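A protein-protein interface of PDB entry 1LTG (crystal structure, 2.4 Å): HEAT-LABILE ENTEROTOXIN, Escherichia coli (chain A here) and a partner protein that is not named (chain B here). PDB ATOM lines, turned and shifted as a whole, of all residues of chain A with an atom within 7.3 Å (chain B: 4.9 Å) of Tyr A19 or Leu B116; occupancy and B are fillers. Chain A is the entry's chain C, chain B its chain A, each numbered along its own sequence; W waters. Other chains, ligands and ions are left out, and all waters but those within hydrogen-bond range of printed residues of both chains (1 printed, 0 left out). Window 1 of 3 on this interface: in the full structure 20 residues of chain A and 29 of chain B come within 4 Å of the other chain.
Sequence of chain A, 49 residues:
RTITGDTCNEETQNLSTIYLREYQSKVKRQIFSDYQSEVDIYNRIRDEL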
ATOM      1  N   GLN A  13      25.074  20.160  18.183  1.00  0.00           N
ATOM      2  CA  GLN A  13      24.481  21.004  19.223  1.00  0.00           C
ATOM      3  C   GLN A  13      22.944  21.075  19.157  1.00  0.00           C
ATOM      4  O   GLN A  13      22.230  21.081  20.171  1.00  0.00           O
ATOM      5  CB  GLN A  13      25.044  22.402  19.090  1.00  0.00           C
ATOM      6  CG  GLN A  13      24.439  23.385  20.062  1.00  0.00           C
ATOM      7  CD  GLN A  13      24.796  23.075  21.496  1.00  0.00           C
ATOM      8  OE1 GLN A  13      25.937  22.692  21.752  1.00  0.00           O
ATOM      9  NE2 GLN A  13      23.876  23.220  22.444  1.00  0.00           N
ATOM     10  N   ASN A  14      22.421  21.133  17.935  1.00  0.00           N
ATOM     11  CA  ASN A  14      20.994  21.208  17.657  1.00  0.00           C
ATOM     12  C   ASN A  14      20.289  19.879  17.873  1.00  0.00           C
ATOM     13  O   ASN A  14      19.253  19.826  18.511  1.00  0.00           O
ATOM     14  CB  ASN A  14      20.840  21.694  16.222  1.00  0.00           C
ATOM     15  CG  ASN A  14      19.448  21.482  15.659  1.00  0.00           C
ATOM     16  OD1 ASN A  14      19.218  20.640  14.789  1.00  0.00           O
ATOM     17  ND2 ASN A  14      18.481  22.246  16.156  1.00  0.00           N
ATOM     18  N   LEU A  15      20.819  18.782  17.388  1.00  0.00           N
ATOM     19  CA  LEU A  15      20.217  17.497  17.552  1.00  0.00           C
ATOM     20  C   LEU A  15      20.225  17.173  19.024  1.00  0.00           C
ATOM     21  O   LEU A  15      19.209  16.730  19.559  1.00  0.00           O
ATOM     22  CB  LEU A  15      21.014  16.477  16.793  1.00  0.00           C
ATOM     23  CG  LEU A  15      21.010  16.539  15.287  1.00  0.00           C
ATOM     24  CD1 LEU A  15      22.247  15.862  14.759  1.00  0.00           C
ATOM     25  CD2 LEU A  15      19.730  15.921  14.781  1.00  0.00           C
ATOM     26  N   SER A  16      21.347  17.428  19.698  1.00  0.00           N
ATOM     27  CA  SER A  16      21.488  17.239  21.132  1.00  0.00           C
ATOM     28  C   SER A  16      20.480  18.034  21.924  1.00  0.00           C
ATOM     29  O   SER A  16      19.796  17.460  22.766  1.00  0.00           O
ATOM     30  CB  SER A  16      22.887  17.644  21.571  1.00  0.00           C
ATOM     31  OG  SER A  16      23.826  16.714  21.059  1.00  0.00           O
ATOM     32  N   THR A  17      20.360  19.337  21.678  1.00  0.00           N
ATOM     33  CA  THR A  17      19.336  20.120  22.333  1.00  0.00           C
ATOM     34  C   THR A  17      17.920  19.617  22.006  1.00  0.00           C
ATOM     35  O   THR A  17      17.095  19.597  22.926  1.00  0.00           O
ATOM     36  CB  THR A  17      19.547  21.534  21.904  1.00  0.00           C
ATOM     37  OG1 THR A  17      20.842  21.879  22.380  1.00  0.00           O
ATOM     38  CG2 THR A  17      18.545  22.485  22.481  1.00  0.00           C
ATOM     39  N   ILE A  18      17.563  19.151  20.797  1.00  0.00           N
ATOM     40  CA  ILE A  18      16.241  18.587  20.545  1.00  0.00           C
ATOM     41  C   ILE A  18      16.061  17.309  21.344  1.00  0.00           C
ATOM     42  O   ILE A  18      14.967  17.022  21.821  1.00  0.00           O
ATOM     43  CB  ILE A  18      16.057  18.302  19.046  1.00  0.00           C
ATOM     44  CG1 ILE A  18      15.854  19.624  18.381  1.00  0.00           C
ATOM     45  CG2 ILE A  18      14.830  17.485  18.722  1.00  0.00           C
ATOM     46  CD1 ILE A  18      15.869  19.532  16.839  1.00  0.00           C
ATOM     47  N   TYR A  19      17.083  16.508  21.527  1.00  0.00           N
ATOM     48  CA  TYR A  19      16.991  15.323  22.353  1.00  0.00           C
ATOM     49  C   TYR A  19      16.620  15.743  23.797  1.00  0.00           C
ATOM     50  O   TYR A  19      15.678  15.225  24.418  1.00  0.00           O
ATOM     51  CB  TYR A  19      18.341  14.635  22.322  1.00  0.00           C
ATOM     52  CG  TYR A  19      18.244  13.259  22.891  1.00  0.00           C
ATOM     53  CD1 TYR A  19      18.217  13.013  24.276  1.00  0.00           C
ATOM     54  CD2 TYR A  19      18.088  12.234  21.976  1.00  0.00           C
ATOM     55  CE1 TYR A  19      18.004  11.702  24.737  1.00  0.00           C
ATOM     56  CE2 TYR A  19      17.883  10.927  22.434  1.00  0.00           C
ATOM     57  CZ  TYR A  19      17.837  10.670  23.808  1.00  0.00           C
ATOM     58  OH  TYR A  19      17.594   9.382  24.187  1.00  0.00           O
ATOM     59  N   LEU A  20      17.380  16.677  24.366  1.00  0.00           N
ATOM     60  CA  LEU A  20      17.133  17.160  25.716  1.00  0.00           C
ATOM     61  C   LEU A  20      15.737  17.770  25.889  1.00  0.00           C
ATOM     62  O   LEU A  20      15.045  17.369  26.830  1.00  0.00           O
ATOM     63  CB  LEU A  20      18.215  18.185  26.102  1.00  0.00           C
ATOM     64  CG  LEU A  20      18.103  18.838  27.482  1.00  0.00           C
ATOM     65  CD1 LEU A  20      18.179  17.798  28.585  1.00  0.00           C
ATOM     66  CD2 LEU A  20      19.219  19.848  27.633  1.00  0.00           C
ATOM     67  N   ARG A  21      15.249  18.684  25.032  1.00  0.00           N
ATOM     68  CA  ARG A  21      13.911  19.273  25.152  1.00  0.00           C
ATOM     69  C   ARG A  21      12.803  18.210  25.151  1.00  0.00           C
ATOM     70  O   ARG A  21      11.826  18.344  25.902  1.00  0.00           O
ATOM     71  CB  ARG A  21      13.613  20.244  24.009  1.00  0.00           C
ATOM     72  CG  ARG A  21      14.452  21.508  23.838  1.00  0.00           C
ATOM     73  CD  ARG A  21      14.340  22.568  24.933  1.00  0.00           C
ATOM     74  NE  ARG A  21      15.512  22.562  25.805  1.00  0.00           N
ATOM     75  CZ  ARG A  21      16.331  23.623  25.950  1.00  0.00           C
ATOM     76  NH1 ARG A  21      16.137  24.784  25.302  1.00  0.00           N
ATOM     77  NH2 ARG A  21      17.386  23.529  26.770  1.00  0.00           N
ATOM     78  N   GLU A  22      12.967  17.108  24.409  1.00  0.00           N
ATOM     79  CA  GLU A  22      11.965  16.036  24.415  1.00  0.00           C
ATOM     80  C   GLU A  22      11.904  15.403  25.793  1.00  0.00           C
ATOM     81  O   GLU A  22      10.825  15.152  26.339  1.00  0.00           O
ATOM     82  CB  GLU A  22      12.250  14.850  23.443  1.00  0.00           C
ATOM     83  CG  GLU A  22      12.293  15.072  21.916  1.00  0.00           C
ATOM     84  CD  GLU A  22      11.062  15.700  21.243  1.00  0.00           C
ATOM     85  OE1 GLU A  22      10.133  14.978  20.861  1.00  0.00           O
ATOM     86  OE2 GLU A  22      11.048  16.923  21.083  1.00  0.00           O
ATOM     87  N   TYR A  23      13.091  15.186  26.364  1.00  0.00           N
ATOM     88  CA  TYR A  23      13.204  14.578  27.654  1.00  0.00           C
ATOM     89  C   TYR A  23      12.593  15.545  28.664  1.00  0.00           C
ATOM     90  O   TYR A  23      11.759  15.114  29.474  1.00  0.00           O
ATOM     91  CB  TYR A  23      14.661  14.291  27.947  1.00  0.00           C
ATOM     92  CG  TYR A  23      14.704  13.380  29.164  1.00  0.00           C
ATOM     93  CD1 TYR A  23      14.203  12.081  29.102  1.00  0.00           C
ATOM     94  CD2 TYR A  23      15.220  13.872  30.363  1.00  0.00           C
ATOM     95  CE1 TYR A  23      14.215  11.275  30.243  1.00  0.00           C
ATOM     96  CE2 TYR A  23      15.236  13.068  31.501  1.00  0.00           C
ATOM     97  CZ  TYR A  23      14.736  11.773  31.433  1.00  0.00           C
ATOM     98  OH  TYR A  23      14.816  10.971  32.556  1.00  0.00           O
ATOM     99  N   GLN A  24      12.854  16.848  28.599  1.00  0.00           N
ATOM    100  CA  GLN A  24      12.257  17.779  29.553  1.00  0.00           C
ATOM    101  C   GLN A  24      10.743  17.810  29.572  1.00  0.00           C
ATOM    102  O   GLN A  24      10.148  17.829  30.653  1.00  0.00           O
ATOM    103  CB  GLN A  24      12.810  19.176  29.303  1.00  0.00           C
ATOM    104  CG  GLN A  24      14.195  19.245  29.984  1.00  0.00           C
ATOM    105  CD  GLN A  24      15.064  20.463  29.738  1.00  0.00           C
ATOM    106  OE1 GLN A  24      15.906  20.816  30.548  1.00  0.00           O
ATOM    107  NE2 GLN A  24      14.980  21.133  28.603  1.00  0.00           N
ATOM    108  N   ILE B  39      26.574  21.170  24.049  1.00  0.00           N
ATOM    109  CA  ILE B  39      26.367  19.767  24.307  1.00  0.00           C
ATOM    110  C   ILE B  39      27.142  18.991  23.263  1.00  0.00           C
ATOM    111  O   ILE B  39      26.757  18.995  22.091  1.00  0.00           O
ATOM    112  CB  ILE B  39      24.882  19.443  24.203  1.00  0.00           C
ATOM    113  CG1 ILE B  39      24.029  20.258  25.170  1.00  0.00           C
ATOM    114  CG2 ILE B  39      24.762  17.960  24.491  1.00  0.00           C
ATOM    115  CD1 ILE B  39      22.515  20.272  24.865  1.00  0.00           C
ATOM    116  N   GLY B  58      28.057  19.901  28.671  1.00  0.00           N
ATOM    117  CA  GLY B  58      26.661  19.596  28.890  1.00  0.00           C
ATOM    118  C   GLY B  58      26.292  18.230  29.440  1.00  0.00           C
ATOM    119  O   GLY B  58      25.095  17.946  29.607  1.00  0.00           O
ATOM    120  N   TYR B  59      27.268  17.394  29.748  1.00  0.00           N
ATOM    121  CA  TYR B  59      26.935  16.084  30.221  1.00  0.00           C
ATOM    122  C   TYR B  59      27.416  16.000  31.643  1.00  0.00           C
ATOM    123  O   TYR B  59      28.348  16.744  31.976  1.00  0.00           O
ATOM    124  CB  TYR B  59      27.626  15.062  29.374  1.00  0.00           C
ATOM    125  CG  TYR B  59      27.061  14.820  27.990  1.00  0.00           C
ATOM    126  CD1 TYR B  59      27.407  15.603  26.892  1.00  0.00           C
ATOM    127  CD2 TYR B  59      26.195  13.736  27.812  1.00  0.00           C
ATOM    128  CE1 TYR B  59      26.879  15.288  25.633  1.00  0.00           C
ATOM    129  CE2 TYR B  59      25.667  13.417  26.547  1.00  0.00           C
ATOM    130  CZ  TYR B  59      26.007  14.196  25.453  1.00  0.00           C
ATOM    131  OH  TYR B  59      25.448  13.881  24.218  1.00  0.00           O
ATOM    132  N   PRO B  92      16.235   7.134  29.476  1.00  0.00           N
ATOM    133  CA  PRO B  92      16.865   7.512  28.222  1.00  0.00           C
ATOM    134  C   PRO B  92      17.675   8.816  28.125  1.00  0.00           C
ATOM    135  O   PRO B  92      18.184   9.136  27.064  1.00  0.00           O
ATOM    136  CB  PRO B  92      15.708   7.416  27.249  1.00  0.00           C
ATOM    137  CG  PRO B  92      14.863   6.327  27.819  1.00  0.00           C
ATOM    138  CD  PRO B  92      14.831   6.810  29.249  1.00  0.00           C
ATOM    139  N   ASN B  93      17.936   9.662  29.112  1.00  0.00           N
ATOM    140  CA  ASN B  93      18.832  10.825  28.918  1.00  0.00           C
ATOM    141  C   ASN B  93      20.274  10.355  29.150  1.00  0.00           C
ATOM    142  O   ASN B  93      21.204  11.158  29.059  1.00  0.00           O
ATOM    143  CB  ASN B  93      18.536  12.014  29.922  1.00  0.00           C
ATOM    144  CG  ASN B  93      18.389  11.618  31.414  1.00  0.00           C
ATOM    145  OD1 ASN B  93      18.107  10.446  31.755  1.00  0.00           O
ATOM    146  ND2 ASN B  93      18.510  12.516  32.383  1.00  0.00           N
ATOM    147  N   PHE B  95      23.590   7.915  28.391  1.00  0.00           N
ATOM    148  CA  PHE B  95      24.240   7.272  27.254  1.00  0.00           C
ATOM    149  C   PHE B  95      25.498   6.543  27.706  1.00  0.00           C
ATOM    150  O   PHE B  95      26.300   7.133  28.454  1.00  0.00           O
ATOM    151  CB  PHE B  95      24.666   8.283  26.257  1.00  0.00           C
ATOM    152  CG  PHE B  95      23.519   8.868  25.525  1.00  0.00           C
ATOM    153  CD1 PHE B  95      23.024   8.208  24.394  1.00  0.00           C
ATOM    154  CD2 PHE B  95      23.016  10.090  25.940  1.00  0.00           C
ATOM    155  CE1 PHE B  95      21.995   8.807  23.650  1.00  0.00           C
ATOM    156  CE2 PHE B  95      21.990  10.674  25.189  1.00  0.00           C
ATOM    157  CZ  PHE B  95      21.482  10.039  24.047  1.00  0.00           C
ATOM    158  N   SER B 114      26.983   8.966  30.632  1.00  0.00           N
ATOM    159  CA  SER B 114      26.684  10.370  30.779  1.00  0.00           C
ATOM    160  C   SER B 114      25.214  10.669  30.574  1.00  0.00           C
ATOM    161  O   SER B 114      24.549  10.024  29.768  1.00  0.00           O
ATOM    162  CB  SER B 114      27.477  11.191  29.774  1.00  0.00           C
ATOM    163  OG  SER B 114      28.841  11.369  30.148  1.00  0.00           O
ATOM    164  N   ALA B 115      24.727  11.660  31.307  1.00  0.00           N
ATOM    165  CA  ALA B 115      23.378  12.155  31.192  1.00  0.00           C
ATOM    166  C   ALA B 115      23.435  13.476  30.488  1.00  0.00           C
ATOM    167  O   ALA B 115      24.171  14.407  30.887  1.00  0.00           O
ATOM    168  CB  ALA B 115      22.744  12.438  32.521  1.00  0.00           C
ATOM    169  N   LEU B 116      22.645  13.528  29.430  1.00  0.00           N
ATOM    170  CA  LEU B 116      22.587  14.753  28.673  1.00  0.00           C
ATOM    171  C   LEU B 116      21.555  15.614  29.370  1.00  0.00           C
ATOM    172  O   LEU B 116      20.401  15.189  29.487  1.00  0.00           O
ATOM    173  CB  LEU B 116      22.205  14.372  27.251  1.00  0.00           C
ATOM    174  CG  LEU B 116      21.551  15.222  26.200  1.00  0.00           C
ATOM    175  CD1 LEU B 116      22.164  16.547  26.065  1.00  0.00           C
ATOM    176  CD2 LEU B 116      21.732  14.485  24.894  1.00  0.00           C
ATOM    177  N   GLY B 117      22.035  16.775  29.842  1.00  0.00           N
ATOM    178  CA  GLY B 117      21.161  17.794  30.400  1.00  0.00           C
ATOM    179  C   GLY B 117      21.341  18.052  31.866  1.00  0.00           C
ATOM    180  O   GLY B 117      21.047  19.140  32.357  1.00  0.00           O
ATOM    181  N   GLY B 118      21.937  17.060  32.508  1.00  0.00           N
ATOM    182  CA  GLY B 118      22.081  17.004  33.942  1.00  0.00           C
ATOM    183  C   GLY B 118      21.172  15.880  34.458  1.00  0.00           C
ATOM    184  O   GLY B 118      20.788  14.994  33.694  1.00  0.00           O
ATOM    185  N   ALA B 156      19.720   5.024  27.083  1.00  0.00           N
ATOM    186  CA  ALA B 156      19.432   5.139  25.667  1.00  0.00           C
ATOM    187  C   ALA B 156      20.288   4.150  24.885  1.00  0.00           C
ATOM    188  O   ALA B 156      21.388   3.830  25.324  1.00  0.00           O
ATOM    189  CB  ALA B 156      19.754   6.525  25.208  1.00  0.00           C
ATOM    190  N   ASP B 160      21.037   5.212  19.012  1.00  0.00           N
ATOM    191  CA  ASP B 160      20.578   6.582  19.142  1.00  0.00           C
ATOM    192  C   ASP B 160      21.705   7.515  19.537  1.00  0.00           C
ATOM    193  O   ASP B 160      21.662   8.744  19.380  1.00  0.00           O
ATOM    194  CB  ASP B 160      19.474   6.635  20.195  1.00  0.00           C
ATOM    195  CG  ASP B 160      18.167   5.928  19.863  1.00  0.00           C
ATOM    196  OD1 ASP B 160      18.038   5.284  18.822  1.00  0.00           O
ATOM    197  OD2 ASP B 160      17.254   6.043  20.671  1.00  0.00           O
ATOM    198  N   ARG B 163      24.399   9.422  16.290  1.00  0.00           N
ATOM    199  CA  ARG B 163      24.180  10.718  15.643  1.00  0.00           C
ATOM    200  C   ARG B 163      24.594  11.890  16.511  1.00  0.00           C
ATOM    201  O   ARG B 163      24.607  13.023  16.031  1.00  0.00           O
ATOM    202  CB  ARG B 163      22.685  10.822  15.267  1.00  0.00           C
ATOM    203  CG  ARG B 163      21.788  12.017  15.653  1.00  0.00           C
ATOM    204  CD  ARG B 163      20.843  11.829  16.890  1.00  0.00           C
ATOM    205  NE  ARG B 163      20.084  13.046  17.281  1.00  0.00           N
ATOM    206  CZ  ARG B 163      18.825  13.050  17.798  1.00  0.00           C
ATOM    207  NH1 ARG B 163      18.139  11.919  18.015  1.00  0.00           N
ATOM    208  NH2 ARG B 163      18.215  14.213  18.085  1.00  0.00           N
ATOM    209  N   LEU B 164      24.786  11.593  17.810  1.00  0.00           N
ATOM    210  CA  LEU B 164      25.099  12.580  18.838  1.00  0.00           C
ATOM    211  C   LEU B 164      26.506  12.544  19.393  1.00  0.00           C
ATOM    212  O   LEU B 164      26.814  13.310  20.316  1.00  0.00           O
ATOM    213  CB  LEU B 164      24.145  12.437  20.035  1.00  0.00           C
ATOM    214  CG  LEU B 164      22.663  12.710  19.897  1.00  0.00           C
ATOM    215  CD1 LEU B 164      22.031  12.640  21.263  1.00  0.00           C
ATOM    216  CD2 LEU B 164      22.414  14.100  19.351  1.00  0.00           C
HETATM  217  O   HOH W   1      16.591   6.680  23.258  1.00  0.00           O
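The side-chain amide oxygen (OE1) of Gln A13 sits at hydrogen-bond distance from the backbone NH (N) of Ile B39 (2.8 Å). The backbone carbonyl oxygen (O) of Pro B92 sits at hydrogen-bond distance from the side-chain hydroxyl (OH) of Tyr A19. The side-chain amide oxygen of Asn B93 sits at hydrogen-bond distance from the side-chain hydroxyl of Tyr A23, 3.4 Å away. The backbone carbonyl oxygen (O) of Leu A15 lies within hydrogen-bond range of the guanidinium group (NH2) of Arg B163.
The backbone NH (N) of Gly B117 lies within hydrogen-bond range of the backbone carbonyl oxygen (O) of Gly B58 (3.3 Å). O of Asn B93 sits at hydrogen-bond distance from N of Leu B116. The backbone carbonyl oxygen of Ser B114 lies within hydrogen-bond range of the backbone NH of Phe B95 (2.7 Å). The side-chain hydroxyl (OG1) of Thr A17 lies within hydrogen-bond range of the backbone carbonyl oxygen (O) of Gln A13 (2.7 Å).
Of chain B, only Pro B92, Phe B95, Leu B116, Ala B156 and Arg B163 come within 4 Å of Tyr A19. Ala B115 touches none of the printed residues of chain A. Leu B116 touches just these residues of chain A: Tyr A19 (3.9 Å) and Leu A20 (3.5 Å). Printed residues of chain A within 4 Å of Gly B117: Leu A20. Of the printed residues of chain A, Leu B164 touches Leu A15 and Ser A16. The nearest printed residue of chain B that does not touch Gln A13 is Leu B164 (6.7 Å).
CD2 of Leu B164 touches CB of Leu A15, 3.8 Å away. CB of Ser A16 touches CG2 of Ile B39, 3.5 Å away. Ser A16 touches Leu B164. Ile B39 touches Thr A17. CZ of Tyr A19 touches CZ of Phe B95 (3.7 Å). CD1 of Tyr A19 touches CD2 of Leu B116, 3.9 Å away. Tyr A19 touches Ala B156. NH1 of Arg B163 touches CD2 of Tyr A19, 3.97 Å away. O of Leu B116 touches CD1 of Leu A20, 3.5 Å away. Leu A20 touches Gly B117 (CD1 to CA, 3.5 Å).
Water W1 lies within hydrogen-bond range of OD2 of Asp B160 (2.7 Å) and OH of Tyr A19 (3.0 Å).
Hydrophobic or aromatic side chains of chain B that line the printed part of chain A: Ile B39, Phe B95, Leu B116, Ala B156 and Leu B164. Printed residues of chain A that touch a printed residue of chain B: Gln A13, Leu A15, Ser A16, Thr A17, Tyr A19, Leu A20 and Tyr A23. Hydrophobic or aromatic side chains of chain A that line the printed part of chain B: Leu A15, Tyr A19, Leu A20 and Tyr A23. Along chain A the printed residues that touch a printed residue of chain B span positions 13 to 23. Among the printed residues, 14 pairs touch across the chains. Among the printed residues, no Asp or Glu carboxylate lies within 4 Å of a Lys or Arg side-chain nitrogen of the other chain.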
